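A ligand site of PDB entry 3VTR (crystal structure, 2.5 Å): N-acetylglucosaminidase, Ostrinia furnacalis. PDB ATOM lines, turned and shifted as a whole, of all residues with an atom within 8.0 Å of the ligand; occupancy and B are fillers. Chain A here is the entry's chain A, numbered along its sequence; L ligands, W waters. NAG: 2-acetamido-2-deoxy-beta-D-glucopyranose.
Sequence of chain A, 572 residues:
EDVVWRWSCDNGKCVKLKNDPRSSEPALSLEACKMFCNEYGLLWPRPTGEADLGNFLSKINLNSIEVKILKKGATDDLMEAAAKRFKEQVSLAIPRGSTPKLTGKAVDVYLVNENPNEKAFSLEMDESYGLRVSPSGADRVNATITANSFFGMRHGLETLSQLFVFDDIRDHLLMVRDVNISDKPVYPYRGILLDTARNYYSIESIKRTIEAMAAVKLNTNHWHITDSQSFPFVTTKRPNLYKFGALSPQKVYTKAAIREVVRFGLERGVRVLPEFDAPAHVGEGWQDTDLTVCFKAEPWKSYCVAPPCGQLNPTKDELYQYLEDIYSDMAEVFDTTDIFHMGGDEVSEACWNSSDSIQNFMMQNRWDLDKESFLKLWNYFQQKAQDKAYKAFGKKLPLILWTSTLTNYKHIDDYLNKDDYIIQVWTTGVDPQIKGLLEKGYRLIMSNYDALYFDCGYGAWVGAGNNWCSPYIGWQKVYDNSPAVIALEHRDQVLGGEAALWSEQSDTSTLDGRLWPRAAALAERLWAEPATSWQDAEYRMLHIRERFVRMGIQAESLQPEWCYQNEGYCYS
The side-chain amide oxygen of Gln 359 sits at hydrogen-bond distance from the side-chain amide nitrogen of Asn 353 (2.7 Å).
Residues that only touch the ligand: Gln 359 (3.6 Å). Within 4 Å of the ligand: Asn 353, Gln 359 and Leu 369. The nearest printed residue that does not touch the ligand is Phe 374 (4.2 Å).
A nitrogen (N2) of the ligand sits at hydrogen-bond distance from the side-chain amide oxygen (OD1) of Asn 353 (2.8 Å). O of Leu 369 is in hydrogen-bond range of N2 of the ligand (3.1 Å).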
ATOM      1  N   GLU A 349      -2.561  33.001 -18.694  1.00  0.00           N
ATOM      2  CA  GLU A 349      -3.031  31.639 -18.425  1.00  0.00           C
ATOM      3  C   GLU A 349      -1.837  30.709 -18.161  1.00  0.00           C
ATOM      4  O   GLU A 349      -1.907  29.850 -17.288  1.00  0.00           O
ATOM      5  CB  GLU A 349      -3.885  31.110 -19.585  1.00  0.00           C
ATOM      6  CG  GLU A 349      -3.356  31.437 -20.981  1.00  0.00           C
ATOM      7  CD  GLU A 349      -3.548  32.900 -21.362  1.00  0.00           C
ATOM      8  OE1 GLU A 349      -4.702  33.348 -21.510  1.00  0.00           O
ATOM      9  OE2 GLU A 349      -2.518  33.609 -21.511  1.00  0.00           O
ATOM     10  N   ALA A 350      -0.759  30.917 -18.916  1.00  0.00           N
ATOM     11  CA  ALA A 350       0.478  30.175 -18.709  1.00  0.00           C
ATOM     12  C   ALA A 350       1.005  30.345 -17.286  1.00  0.00           C
ATOM     13  O   ALA A 350       1.454  29.383 -16.664  1.00  0.00           O
ATOM     14  CB  ALA A 350       1.543  30.602 -19.725  1.00  0.00           C
ATOM     15  N   CYS A 351       0.939  31.575 -16.787  1.00  0.00           N
ATOM     16  CA  CYS A 351       1.396  31.867 -15.440  1.00  0.00           C
ATOM     17  C   CYS A 351       0.647  31.071 -14.387  1.00  0.00           C
ATOM     18  O   CYS A 351       1.269  30.394 -13.561  1.00  0.00           O
ATOM     19  CB  CYS A 351       1.260  33.350 -15.152  1.00  0.00           C
ATOM     20  SG  CYS A 351       2.082  33.842 -13.613  1.00  0.00           S
ATOM     21  N   TRP A 352      -0.678  31.144 -14.411  1.00  0.00           N
ATOM     22  CA  TRP A 352      -1.506  30.401 -13.453  1.00  0.00           C
ATOM     23  C   TRP A 352      -1.350  28.900 -13.615  1.00  0.00           C
ATOM     24  O   TRP A 352      -1.472  28.144 -12.647  1.00  0.00           O
ATOM     25  CB  TRP A 352      -2.975  30.797 -13.563  1.00  0.00           C
ATOM     26  CG  TRP A 352      -3.325  32.054 -12.817  1.00  0.00           C
ATOM     27  CD1 TRP A 352      -2.546  32.702 -11.890  1.00  0.00           C
ATOM     28  CD2 TRP A 352      -4.555  32.793 -12.891  1.00  0.00           C
ATOM     29  NE1 TRP A 352      -3.204  33.811 -11.406  1.00  0.00           N
ATOM     30  CE2 TRP A 352      -4.439  33.890 -12.002  1.00  0.00           C
ATOM     31  CE3 TRP A 352      -5.726  32.647 -13.628  1.00  0.00           C
ATOM     32  CZ2 TRP A 352      -5.456  34.830 -11.838  1.00  0.00           C
ATOM     33  CZ3 TRP A 352      -6.748  33.580 -13.458  1.00  0.00           C
ATOM     34  CH2 TRP A 352      -6.600  34.660 -12.567  1.00  0.00           C
ATOM     35  N   ASN A 353      -1.079  28.449 -14.836  1.00  0.00           N
ATOM     36  CA  ASN A 353      -0.989  27.020 -15.111  1.00  0.00           C
ATOM     37  C   ASN A 353       0.348  26.393 -14.709  1.00  0.00           C
ATOM     38  O   ASN A 353       0.469  25.163 -14.709  1.00  0.00           O
ATOM     39  CB  ASN A 353      -1.301  26.728 -16.572  1.00  0.00           C
ATOM     40  CG  ASN A 353      -2.115  25.468 -16.740  1.00  0.00           C
ATOM     41  OD1 ASN A 353      -2.949  25.366 -17.640  1.00  0.00           O
ATOM     42  ND2 ASN A 353      -1.904  24.485 -15.860  1.00  0.00           N
ATOM     43  N   SER A 354       1.332  27.220 -14.380  1.00  0.00           N
ATOM     44  CA  SER A 354       2.645  26.709 -13.995  1.00  0.00           C
ATOM     45  C   SER A 354       2.747  26.440 -12.480  1.00  0.00           C
ATOM     46  O   SER A 354       3.803  26.040 -12.000  1.00  0.00           O
ATOM     47  CB  SER A 354       3.762  27.662 -14.455  1.00  0.00           C
ATOM     48  OG  SER A 354       3.924  28.747 -13.549  1.00  0.00           O
ATOM     49  N   GLN A 359      -3.396  24.364 -10.009  1.00  0.00           N
ATOM     50  CA  GLN A 359      -3.917  23.201 -10.722  1.00  0.00           C
ATOM     51  C   GLN A 359      -4.688  22.253  -9.788  1.00  0.00           C
ATOM     52  O   GLN A 359      -5.745  21.754 -10.164  1.00  0.00           O
ATOM     53  CB  GLN A 359      -2.797  22.451 -11.444  1.00  0.00           C
ATOM     54  CG  GLN A 359      -2.375  23.108 -12.744  1.00  0.00           C
ATOM     55  CD  GLN A 359      -1.170  22.432 -13.375  1.00  0.00           C
ATOM     56  OE1 GLN A 359      -1.129  22.219 -14.587  1.00  0.00           O
ATOM     57  NE2 GLN A 359      -0.179  22.092 -12.561  1.00  0.00           N
ATOM     58  N   ASP A 368     -11.342  22.459 -15.583  1.00  0.00           N
ATOM     59  CA  ASP A 368     -10.282  21.844 -16.312  1.00  0.00           C
ATOM     60  C   ASP A 368      -9.051  22.735 -16.351  1.00  0.00           C
ATOM     61  O   ASP A 368      -8.955  23.709 -15.597  1.00  0.00           O
ATOM     62  CB  ASP A 368     -10.752  21.432 -17.702  1.00  0.00           C
ATOM     63  CG  ASP A 368     -11.728  20.271 -17.640  1.00  0.00           C
ATOM     64  OD1 ASP A 368     -12.704  20.343 -16.864  1.00  0.00           O
ATOM     65  OD2 ASP A 368     -11.523  19.271 -18.363  1.00  0.00           O
ATOM     66  N   LEU A 369      -8.104  22.382 -17.195  1.00  0.00           N
ATOM     67  CA  LEU A 369      -6.927  23.210 -17.357  1.00  0.00           C
ATOM     68  C   LEU A 369      -6.985  23.963 -18.684  1.00  0.00           C
ATOM     69  O   LEU A 369      -5.953  24.414 -19.201  1.00  0.00           O
ATOM     70  CB  LEU A 369      -5.655  22.380 -17.191  1.00  0.00           C
ATOM     71  CG  LEU A 369      -5.471  21.762 -15.793  1.00  0.00           C
ATOM     72  CD1 LEU A 369      -4.196  20.926 -15.715  1.00  0.00           C
ATOM     73  CD2 LEU A 369      -5.499  22.829 -14.692  1.00  0.00           C
ATOM     74  N   ASP A 370      -8.213  24.111 -19.215  1.00  0.00           N
ATOM     75  CA  ASP A 370      -8.455  24.896 -20.434  1.00  0.00           C
ATOM     76  C   ASP A 370      -8.672  26.388 -20.144  1.00  0.00           C
ATOM     77  O   ASP A 370      -8.491  26.834 -19.013  1.00  0.00           O
ATOM     78  CB  ASP A 370      -9.609  24.294 -21.256  1.00  0.00           C
ATOM     79  CG  ASP A 370     -10.926  24.226 -20.477  1.00  0.00           C
ATOM     80  OD1 ASP A 370     -11.920  23.731 -21.069  1.00  0.00           O
ATOM     81  OD2 ASP A 370     -10.979  24.647 -19.304  1.00  0.00           O
ATOM     82  N   LYS A 371      -9.070  27.130 -21.173  1.00  0.00           N
ATOM     83  CA  LYS A 371      -9.197  28.594 -21.114  1.00  0.00           C
ATOM     84  C   LYS A 371     -10.352  29.089 -20.238  1.00  0.00           C
ATOM     85  O   LYS A 371     -10.136  29.927 -19.356  1.00  0.00           O
ATOM     86  CB  LYS A 371      -9.367  29.160 -22.526  1.00  0.00           C
ATOM     87  CG  LYS A 371      -8.261  28.785 -23.516  1.00  0.00           C
ATOM     88  CD  LYS A 371      -7.432  29.990 -23.944  1.00  0.00           C
ATOM     89  CE  LYS A 371      -6.399  30.388 -22.906  1.00  0.00           C
ATOM     90  NZ  LYS A 371      -5.829  31.719 -23.257  1.00  0.00           N
ATOM     91  N   GLU A 372     -11.553  28.576 -20.483  1.00  0.00           N
ATOM     92  CA  GLU A 372     -12.767  29.038 -19.799  1.00  0.00           C
ATOM     93  C   GLU A 372     -12.672  28.820 -18.282  1.00  0.00           C
ATOM     94  O   GLU A 372     -13.305  29.552 -17.508  1.00  0.00           O
ATOM     95  CB  GLU A 372     -14.003  28.327 -20.353  1.00  0.00           C
ATOM     96  CG  GLU A 372     -15.322  29.094 -20.178  1.00  0.00           C
ATOM     97  CD  GLU A 372     -15.559  30.139 -21.269  1.00  0.00           C
ATOM     98  OE1 GLU A 372     -16.485  30.963 -21.106  1.00  0.00           O
ATOM     99  OE2 GLU A 372     -14.843  30.127 -22.288  1.00  0.00           O
ATOM    100  N   SER A 373     -11.882  27.832 -17.882  1.00  0.00           N
ATOM    101  CA  SER A 373     -11.676  27.531 -16.478  1.00  0.00           C
ATOM    102  C   SER A 373     -10.761  28.553 -15.799  1.00  0.00           C
ATOM    103  O   SER A 373     -10.994  28.923 -14.643  1.00  0.00           O
ATOM    104  CB  SER A 373     -11.139  26.105 -16.296  1.00  0.00           C
ATOM    105  OG  SER A 373     -10.063  25.831 -17.209  1.00  0.00           O
ATOM    106  N   PHE A 374      -9.718  28.991 -16.504  1.00  0.00           N
ATOM    107  CA  PHE A 374      -8.865  30.065 -15.992  1.00  0.00           C
ATOM    108  C   PHE A 374      -9.610  31.390 -15.968  1.00  0.00           C
ATOM    109  O   PHE A 374      -9.326  32.257 -15.139  1.00  0.00           O
ATOM    110  CB  PHE A 374      -7.554  30.162 -16.775  1.00  0.00           C
ATOM    111  CG  PHE A 374      -6.592  29.071 -16.438  1.00  0.00           C
ATOM    112  CD1 PHE A 374      -5.946  29.053 -15.207  1.00  0.00           C
ATOM    113  CD2 PHE A 374      -6.338  28.047 -17.336  1.00  0.00           C
ATOM    114  CE1 PHE A 374      -5.046  28.047 -14.884  1.00  0.00           C
ATOM    115  CE2 PHE A 374      -5.458  27.029 -17.022  1.00  0.00           C
ATOM    116  CZ  PHE A 374      -4.810  27.025 -15.791  1.00  0.00           C
HETATM  117  C1  NAG L   1      -1.219  23.231 -18.692  1.00  0.00           C
HETATM  118  C2  NAG L   1      -2.040  23.070 -19.979  1.00  0.00           C
HETATM  119  C3  NAG L   1      -2.726  21.709 -20.087  1.00  0.00           C
HETATM  120  C4  NAG L   1      -1.700  20.619 -19.803  1.00  0.00           C
HETATM  121  C5  NAG L   1      -1.232  20.788 -18.356  1.00  0.00           C
HETATM  122  C6  NAG L   1      -0.235  19.699 -17.959  1.00  0.00           C
HETATM  123  C7  NAG L   1      -2.823  25.293 -20.729  1.00  0.00           C
HETATM  124  C8  NAG L   1      -4.079  26.285 -20.868  1.00  0.00           C
HETATM  125  N2  NAG L   1      -3.063  24.101 -20.178  1.00  0.00           N
HETATM  126  O3  NAG L   1      -3.253  21.551 -21.382  1.00  0.00           O
HETATM  127  O4  NAG L   1      -2.272  19.347 -20.014  1.00  0.00           O
HETATM  128  O5  NAG L   1      -0.609  22.047 -18.157  1.00  0.00           O
HETATM  129  O6  NAG L   1       0.737  20.220 -17.073  1.00  0.00           O
HETATM  130  O7  NAG L   1      -1.653  25.620 -21.107  1.00  0.00           O
HETATM  131  O   HOH W   1      -5.130  19.731 -22.031  1.00  0.00           O
